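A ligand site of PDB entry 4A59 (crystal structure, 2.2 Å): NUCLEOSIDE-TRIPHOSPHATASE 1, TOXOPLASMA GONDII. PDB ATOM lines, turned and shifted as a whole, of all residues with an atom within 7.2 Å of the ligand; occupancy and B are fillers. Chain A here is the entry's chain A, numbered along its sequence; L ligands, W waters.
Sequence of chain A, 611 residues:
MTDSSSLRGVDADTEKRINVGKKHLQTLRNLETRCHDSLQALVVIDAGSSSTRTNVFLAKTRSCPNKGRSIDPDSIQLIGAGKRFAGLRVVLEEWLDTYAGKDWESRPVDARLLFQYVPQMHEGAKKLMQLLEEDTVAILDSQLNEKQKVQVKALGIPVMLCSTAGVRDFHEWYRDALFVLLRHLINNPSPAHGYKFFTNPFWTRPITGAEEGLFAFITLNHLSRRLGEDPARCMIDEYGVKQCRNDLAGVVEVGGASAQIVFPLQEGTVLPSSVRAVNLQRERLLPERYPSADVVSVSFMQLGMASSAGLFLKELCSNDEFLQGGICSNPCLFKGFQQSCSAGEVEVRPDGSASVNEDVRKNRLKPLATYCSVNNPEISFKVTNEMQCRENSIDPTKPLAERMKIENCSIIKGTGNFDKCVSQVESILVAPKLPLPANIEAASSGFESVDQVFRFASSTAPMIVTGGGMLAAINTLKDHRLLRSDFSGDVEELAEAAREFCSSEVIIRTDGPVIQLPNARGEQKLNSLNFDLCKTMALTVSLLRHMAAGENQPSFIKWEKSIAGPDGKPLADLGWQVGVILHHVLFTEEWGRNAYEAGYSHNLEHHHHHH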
ATOM      1  N   SER A  50     -28.911 -11.023   1.614  1.00  0.00           N
ATOM      2  CA  SER A  50     -30.343 -10.742   1.821  1.00  0.00           C
ATOM      3  C   SER A  50     -30.999  -9.948   0.722  1.00  0.00           C
ATOM      4  O   SER A  50     -32.225  -9.922   0.631  1.00  0.00           O
ATOM      5  CB  SER A  50     -30.563 -10.054   3.167  1.00  0.00           C
ATOM      6  OG  SER A  50     -30.130 -10.899   4.222  1.00  0.00           O
ATOM      7  N   ARG A  84     -33.908  -2.500  -2.648  1.00  0.00           N
ATOM      8  CA  ARG A  84     -33.416  -3.826  -2.285  1.00  0.00           C
ATOM      9  C   ARG A  84     -34.347  -4.835  -2.931  1.00  0.00           C
ATOM     10  O   ARG A  84     -35.542  -4.855  -2.625  1.00  0.00           O
ATOM     11  CB  ARG A  84     -33.352  -4.031  -0.752  1.00  0.00           C
ATOM     12  CG  ARG A  84     -32.299  -3.139  -0.111  1.00  0.00           C
ATOM     13  CD  ARG A  84     -31.931  -3.552   1.291  1.00  0.00           C
ATOM     14  NE  ARG A  84     -31.473  -2.403   2.093  1.00  0.00           N
ATOM     15  CZ  ARG A  84     -30.230  -1.938   2.107  1.00  0.00           C
ATOM     16  NH1 ARG A  84     -29.292  -2.501   1.359  1.00  0.00           N
ATOM     17  NH2 ARG A  84     -29.925  -0.892   2.862  1.00  0.00           N
ATOM     18  N   GLU A 253     -14.455  -4.381   9.452  1.00  0.00           N
ATOM     19  CA  GLU A 253     -15.799  -4.300   8.897  1.00  0.00           C
ATOM     20  C   GLU A 253     -16.651  -5.461   9.404  1.00  0.00           C
ATOM     21  O   GLU A 253     -16.358  -6.615   9.122  1.00  0.00           O
ATOM     22  CB  GLU A 253     -15.768  -4.243   7.359  1.00  0.00           C
ATOM     23  CG  GLU A 253     -17.078  -3.825   6.706  1.00  0.00           C
ATOM     24  CD  GLU A 253     -16.922  -3.080   5.392  1.00  0.00           C
ATOM     25  OE1 GLU A 253     -16.824  -1.826   5.420  1.00  0.00           O
ATOM     26  OE2 GLU A 253     -16.889  -3.747   4.338  1.00  0.00           O
ATOM     27  N   VAL A 254     -17.685  -5.151  10.187  1.00  0.00           N
ATOM     28  CA  VAL A 254     -18.578  -6.183  10.703  1.00  0.00           C
ATOM     29  C   VAL A 254     -19.894  -6.135   9.890  1.00  0.00           C
ATOM     30  O   VAL A 254     -20.722  -5.237  10.089  1.00  0.00           O
ATOM     31  CB  VAL A 254     -18.750  -6.174  12.256  1.00  0.00           C
ATOM     32  CG1 VAL A 254     -19.607  -7.358  12.724  1.00  0.00           C
ATOM     33  CG2 VAL A 254     -17.390  -6.241  12.947  1.00  0.00           C
ATOM     34  N   GLY A 255     -20.022  -7.046   8.934  1.00  0.00           N
ATOM     35  CA  GLY A 255     -21.224  -7.153   8.125  1.00  0.00           C
ATOM     36  C   GLY A 255     -22.202  -8.130   8.747  1.00  0.00           C
ATOM     37  O   GLY A 255     -21.917  -8.715   9.795  1.00  0.00           O
ATOM     38  N   GLY A 256     -23.326  -8.324   8.086  1.00  0.00           N
ATOM     39  CA  GLY A 256     -24.330  -9.297   8.530  1.00  0.00           C
ATOM     40  C   GLY A 256     -23.857 -10.721   8.381  1.00  0.00           C
ATOM     41  O   GLY A 256     -24.117 -11.562   9.252  1.00  0.00           O
ATOM     42  N   ALA A 257     -23.109 -11.006   7.304  1.00  0.00           N
ATOM     43  CA  ALA A 257     -22.649 -12.362   6.949  1.00  0.00           C
ATOM     44  C   ALA A 257     -21.220 -12.724   7.382  1.00  0.00           C
ATOM     45  O   ALA A 257     -20.928 -13.895   7.619  1.00  0.00           O
ATOM     46  CB  ALA A 257     -22.845 -12.605   5.468  1.00  0.00           C
ATOM     47  N   GLY A 304     -19.715 -12.335  11.588  1.00  0.00           N
ATOM     48  CA  GLY A 304     -20.761 -11.547  10.958  1.00  0.00           C
ATOM     49  C   GLY A 304     -21.902 -11.463  11.954  1.00  0.00           C
ATOM     50  O   GLY A 304     -22.001 -12.333  12.828  1.00  0.00           O
ATOM     51  N   MET A 305     -22.731 -10.414  11.879  1.00  0.00           N
ATOM     52  CA  MET A 305     -23.820 -10.245  12.844  1.00  0.00           C
ATOM     53  C   MET A 305     -24.743 -11.485  12.959  1.00  0.00           C
ATOM     54  O   MET A 305     -25.023 -11.898  14.073  1.00  0.00           O
ATOM     55  CB  MET A 305     -24.628  -8.971  12.558  1.00  0.00           C
ATOM     56  CG  MET A 305     -23.771  -7.673  12.556  1.00  0.00           C
ATOM     57  SD  MET A 305     -23.188  -7.186  14.214  1.00  0.00           S
ATOM     58  CE  MET A 305     -24.767  -6.862  15.033  1.00  0.00           C
ATOM     59  N   ALA A 306     -25.175 -12.075  11.839  1.00  0.00           N
ATOM     60  CA  ALA A 306     -26.054 -13.241  11.857  1.00  0.00           C
ATOM     61  C   ALA A 306     -25.418 -14.535  12.408  1.00  0.00           C
ATOM     62  O   ALA A 306     -25.931 -15.118  13.368  1.00  0.00           O
ATOM     63  CB  ALA A 306     -26.656 -13.477  10.478  1.00  0.00           C
ATOM     64  N   THR A 466     -16.148  -0.265  11.086  1.00  0.00           N
ATOM     65  CA  THR A 466     -17.364  -0.043  10.288  1.00  0.00           C
ATOM     66  C   THR A 466     -18.366  -1.195  10.478  1.00  0.00           C
ATOM     67  O   THR A 466     -18.004  -2.278  10.914  1.00  0.00           O
ATOM     68  CB  THR A 466     -17.031   0.220   8.784  1.00  0.00           C
ATOM     69  OG1 THR A 466     -16.604  -1.004   8.161  1.00  0.00           O
ATOM     70  CG2 THR A 466     -15.989   1.301   8.599  1.00  0.00           C
ATOM     71  N   GLY A 467     -19.594  -0.942  10.055  1.00  0.00           N
ATOM     72  CA  GLY A 467     -20.727  -1.850  10.162  1.00  0.00           C
ATOM     73  C   GLY A 467     -21.791  -1.224  11.042  1.00  0.00           C
ATOM     74  O   GLY A 467     -21.469  -0.623  12.073  1.00  0.00           O
ATOM     75  N   GLY A 468     -23.050  -1.367  10.637  1.00  0.00           N
ATOM     76  CA  GLY A 468     -24.220  -0.826  11.327  1.00  0.00           C
ATOM     77  C   GLY A 468     -24.407  -1.254  12.772  1.00  0.00           C
ATOM     78  O   GLY A 468     -24.779  -0.415  13.597  1.00  0.00           O
ATOM     79  N   GLY A 469     -24.165  -2.532  13.069  1.00  0.00           N
ATOM     80  CA  GLY A 469     -24.279  -3.052  14.426  1.00  0.00           C
ATOM     81  C   GLY A 469     -23.168  -2.527  15.321  1.00  0.00           C
ATOM     82  O   GLY A 469     -23.409  -2.195  16.485  1.00  0.00           O
ATOM     83  N   MET A 470     -21.940  -2.405  14.782  1.00  0.00           N
ATOM     84  CA  MET A 470     -20.780  -1.886  15.529  1.00  0.00           C
ATOM     85  C   MET A 470     -21.008  -0.432  15.917  1.00  0.00           C
ATOM     86  O   MET A 470     -20.750  -0.066  17.068  1.00  0.00           O
ATOM     87  CB  MET A 470     -19.476  -2.036  14.739  1.00  0.00           C
ATOM     88  CG  MET A 470     -19.061  -3.485  14.488  1.00  0.00           C
ATOM     89  SD  MET A 470     -18.685  -4.420  15.998  1.00  0.00           S
ATOM     90  CE  MET A 470     -16.993  -3.876  16.356  1.00  0.00           C
ATOM     91  N   LEU A 471     -21.533   0.380  14.961  1.00  0.00           N
ATOM     92  CA  LEU A 471     -21.847   1.787  15.209  1.00  0.00           C
ATOM     93  C   LEU A 471     -23.052   1.992  16.129  1.00  0.00           C
ATOM     94  O   LEU A 471     -23.014   2.868  16.986  1.00  0.00           O
ATOM     95  CB  LEU A 471     -21.948   2.587  13.913  1.00  0.00           C
ATOM     96  CG  LEU A 471     -20.605   3.171  13.490  1.00  0.00           C
ATOM     97  CD1 LEU A 471     -19.904   2.280  12.526  1.00  0.00           C
ATOM     98  CD2 LEU A 471     -20.751   4.544  12.996  1.00  0.00           C
ATOM     99  N   ALA A 472     -24.093   1.154  16.001  1.00  0.00           N
ATOM    100  CA  ALA A 472     -25.257   1.192  16.891  1.00  0.00           C
ATOM    101  C   ALA A 472     -24.819   0.897  18.327  1.00  0.00           C
ATOM    102  O   ALA A 472     -25.340   1.528  19.231  1.00  0.00           O
ATOM    103  CB  ALA A 472     -26.312   0.188  16.454  1.00  0.00           C
ATOM    104  N   ALA A 473     -23.862  -0.029  18.544  1.00  0.00           N
ATOM    105  CA  ALA A 473     -23.341  -0.332  19.890  1.00  0.00           C
ATOM    106  C   ALA A 473     -22.772   0.916  20.545  1.00  0.00           C
ATOM    107  O   ALA A 473     -23.113   1.213  21.671  1.00  0.00           O
ATOM    108  CB  ALA A 473     -22.305  -1.448  19.819  1.00  0.00           C
ATOM    109  N   THR A 476     -25.692   3.971  20.757  1.00  0.00           N
ATOM    110  CA  THR A 476     -26.649   3.651  21.831  1.00  0.00           C
ATOM    111  C   THR A 476     -26.147   4.181  23.177  1.00  0.00           C
ATOM    112  O   THR A 476     -26.928   4.794  23.912  1.00  0.00           O
ATOM    113  CB  THR A 476     -26.936   2.139  21.861  1.00  0.00           C
ATOM    114  OG1 THR A 476     -27.648   1.820  20.681  1.00  0.00           O
ATOM    115  CG2 THR A 476     -27.777   1.728  23.066  1.00  0.00           C
ATOM    116  N   ASN A 527     -36.555  -3.984  20.660  1.00  0.00           N
ATOM    117  CA  ASN A 527     -36.948  -4.458  19.349  1.00  0.00           C
ATOM    118  C   ASN A 527     -36.036  -5.570  18.883  1.00  0.00           C
ATOM    119  O   ASN A 527     -35.072  -5.920  19.562  1.00  0.00           O
ATOM    120  CB  ASN A 527     -37.061  -3.311  18.304  1.00  0.00           C
ATOM    121  CG  ASN A 527     -35.821  -2.458  18.089  1.00  0.00           C
ATOM    122  OD1 ASN A 527     -34.692  -2.944  17.913  1.00  0.00           O
ATOM    123  ND2 ASN A 527     -36.039  -1.163  18.030  1.00  0.00           N
ATOM    124  N   SER A 528     -36.369  -6.133  17.713  1.00  0.00           N
ATOM    125  CA  SER A 528     -35.694  -7.255  17.072  1.00  0.00           C
ATOM    126  C   SER A 528     -34.261  -6.936  16.702  1.00  0.00           C
ATOM    127  O   SER A 528     -33.418  -7.829  16.675  1.00  0.00           O
ATOM    128  CB  SER A 528     -36.491  -7.706  15.847  1.00  0.00           C
ATOM    129  OG  SER A 528     -37.816  -8.033  16.248  1.00  0.00           O
ATOM    130  N   LEU A 529     -33.967  -5.655  16.483  1.00  0.00           N
ATOM    131  CA  LEU A 529     -32.637  -5.228  16.095  1.00  0.00           C
ATOM    132  C   LEU A 529     -31.683  -5.017  17.257  1.00  0.00           C
ATOM    133  O   LEU A 529     -30.495  -5.272  17.105  1.00  0.00           O
ATOM    134  CB  LEU A 529     -32.787  -3.945  15.270  1.00  0.00           C
ATOM    135  CG  LEU A 529     -31.744  -3.663  14.207  1.00  0.00           C
ATOM    136  CD1 LEU A 529     -31.603  -4.854  13.187  1.00  0.00           C
ATOM    137  CD2 LEU A 529     -32.081  -2.330  13.476  1.00  0.00           C
ATOM    138  N   ASN A 530     -32.183  -4.526  18.405  1.00  0.00           N
ATOM    139  CA  ASN A 530     -31.358  -4.156  19.544  1.00  0.00           C
ATOM    140  C   ASN A 530     -31.349  -5.128  20.738  1.00  0.00           C
ATOM    141  O   ASN A 530     -30.559  -4.897  21.653  1.00  0.00           O
ATOM    142  CB  ASN A 530     -31.735  -2.722  20.005  1.00  0.00           C
ATOM    143  CG  ASN A 530     -33.061  -2.525  20.715  1.00  0.00           C
ATOM    144  OD1 ASN A 530     -33.699  -3.459  21.228  1.00  0.00           O
ATOM    145  ND2 ASN A 530     -33.510  -1.290  20.801  1.00  0.00           N
ATOM    146  N   ASP A 532     -30.224  -8.065  21.398  1.00  0.00           N
ATOM    147  CA  ASP A 532     -28.965  -8.757  21.674  1.00  0.00           C
ATOM    148  C   ASP A 532     -27.744  -7.888  21.413  1.00  0.00           C
ATOM    149  O   ASP A 532     -26.648  -8.411  21.349  1.00  0.00           O
ATOM    150  CB  ASP A 532     -28.888 -10.080  20.896  1.00  0.00           C
ATOM    151  CG  ASP A 532     -28.935  -9.946  19.370  1.00  0.00           C
ATOM    152  OD1 ASP A 532     -29.287  -8.853  18.869  1.00  0.00           O
ATOM    153  OD2 ASP A 532     -28.692 -10.963  18.678  1.00  0.00           O
ATOM    154  N   LEU A 533     -27.928  -6.567  21.369  1.00  0.00           N
ATOM    155  CA  LEU A 533     -26.848  -5.594  21.111  1.00  0.00           C
ATOM    156  C   LEU A 533     -25.639  -5.652  22.088  1.00  0.00           C
ATOM    157  O   LEU A 533     -24.512  -5.348  21.686  1.00  0.00           O
ATOM    158  CB  LEU A 533     -27.434  -4.176  20.995  1.00  0.00           C
ATOM    159  CG  LEU A 533     -26.558  -3.101  20.324  1.00  0.00           C
ATOM    160  CD1 LEU A 533     -26.213  -3.495  18.873  1.00  0.00           C
ATOM    161  CD2 LEU A 533     -27.277  -1.763  20.319  1.00  0.00           C
ATOM    162  N   THR A 536     -22.565  -7.426  20.809  1.00  0.00           N
ATOM    163  CA  THR A 536     -21.764  -6.558  19.932  1.00  0.00           C
ATOM    164  C   THR A 536     -20.905  -5.571  20.737  1.00  0.00           C
ATOM    165  O   THR A 536     -19.758  -5.322  20.360  1.00  0.00           O
ATOM    166  CB  THR A 536     -22.694  -5.862  18.896  1.00  0.00           C
ATOM    167  OG1 THR A 536     -23.473  -6.862  18.237  1.00  0.00           O
ATOM    168  CG2 THR A 536     -21.926  -5.068  17.829  1.00  0.00           C
HETATM  169  P1  LIG L   1     -24.900  -2.701   7.595  1.00  0.00           P
HETATM  170  O1  LIG L   1     -25.906  -1.611   7.462  1.00  0.00           O
HETATM  171  O2  LIG L   1     -24.729  -3.544   6.326  1.00  0.00           O
HETATM  172  O3  LIG L   1     -23.534  -2.146   7.938  1.00  0.00           O
HETATM  173  O4  LIG L   1     -25.411  -3.644   8.807  1.00  0.00           O
HETATM  174  C1  LIG L   1     -24.574  -4.783   9.115  1.00  0.00           C
HETATM  175  C2  LIG L   1     -25.346  -5.592  10.107  1.00  0.00           C
HETATM  176  O5  LIG L   1     -25.403  -4.905  11.380  1.00  0.00           O
HETATM  177  C3  LIG L   1     -26.822  -5.789   9.672  1.00  0.00           C
HETATM  178  O6  LIG L   1     -26.887  -6.942   8.874  1.00  0.00           O
HETATM  179  C4  LIG L   1     -27.603  -5.925  10.975  1.00  0.00           C
HETATM  180  O7  LIG L   1     -27.324  -7.245  11.525  1.00  0.00           O
HETATM  181  C5  LIG L   1     -26.792  -4.990  11.880  1.00  0.00           C
HETATM  182  N1  LIG L   1     -27.288  -3.687  12.015  1.00  0.00           N
HETATM  183  C6  LIG L   1     -27.432  -2.663  11.077  1.00  0.00           C
HETATM  184  N2  LIG L   1     -27.922  -1.524  11.637  1.00  0.00           N
HETATM  185  C7  LIG L   1     -28.115  -1.890  12.981  1.00  0.00           C
HETATM  186  C8  LIG L   1     -28.584  -1.201  14.121  1.00  0.00           C
HETATM  187  N3  LIG L   1     -28.962   0.093  14.035  1.00  0.00           N
HETATM  188  N4  LIG L   1     -28.676  -1.860  15.342  1.00  0.00           N
HETATM  189  C9  LIG L   1     -28.270  -3.141  15.434  1.00  0.00           C
HETATM  190  N5  LIG L   1     -27.773  -3.902  14.395  1.00  0.00           N
HETATM  191  C10 LIG L   1     -27.719  -3.218  13.219  1.00  0.00           C
HETATM  192  O   HOH W   1     -28.476  -6.448  15.200  1.00  0.00           O
HETATM  193  O   HOH W   2     -23.681  -6.170   5.927  1.00  0.00           O
HETATM  194  O   HOH W   3     -27.652  -5.163   5.767  1.00  0.00           O
HETATM  195  O   HOH W   4     -28.259   1.936  12.007  1.00  0.00           O
HETATM  196  O   HOH W   5     -27.552  -9.812   9.810  1.00  0.00           O
HETATM  197  O   HOH W   6     -30.189  -0.740  17.881  1.00  0.00           O
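Water W1 lies within hydrogen-bond range of a nitrogen (N5) of the ligand (2.8 Å) and the backbone carbonyl oxygen of Leu 529 (3.0 Å). Water W2 bridges an oxygen (O2) of the ligand (2.9 Å) and the backbone NH of Gly 256 (3.1 Å).
An oxygen (O5) of the ligand lies within hydrogen-bond range of the backbone NH (N) of Gly 469 (3.2 Å). N of Gly 468 is in hydrogen-bond range of O3 of the ligand.
The backbone carbonyl oxygen of Gly 256 sits at hydrogen-bond distance from the backbone NH of Ala 306, 2.8 Å away. The backbone NH (N) of Val 254 is in hydrogen-bond range of the backbone carbonyl oxygen (O) of Thr 466 (3.0 Å). OD1 of Asn 527 sits at hydrogen-bond distance from N of Leu 529, at 3.1 Å. The backbone NH (N) of Met 305 sits at hydrogen-bond distance from the backbone carbonyl oxygen (O) of Gly 256 (3.2 Å). The side-chain hydroxyl of Thr 476 sits at hydrogen-bond distance from the backbone carbonyl oxygen of Ala 472 (2.7 Å). The backbone carbonyl oxygen (O) of Gly 255 sits at hydrogen-bond distance from the backbone NH (N) of Met 305 (2.8 Å).
Residues that only touch the ligand: Val 254 (3.999 Å), Gly 256 (3.5 Å), Met 305 (3.4 Å), Gly 467 (3.6 Å), Ala 472 (3.3 Å) and Leu 529 (3.5 Å). Hydrophobic or aromatic side chains within 4 Å of the ligand: Met 305, Ala 472 and Leu 529. Within 4 Å of the ligand: Val 254, Gly 256, Met 305, Gly 467, Gly 468, Gly 469, Ala 472 and Leu 529. The nearest printed residue that does not touch the ligand is Leu 533 (4.02 Å).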
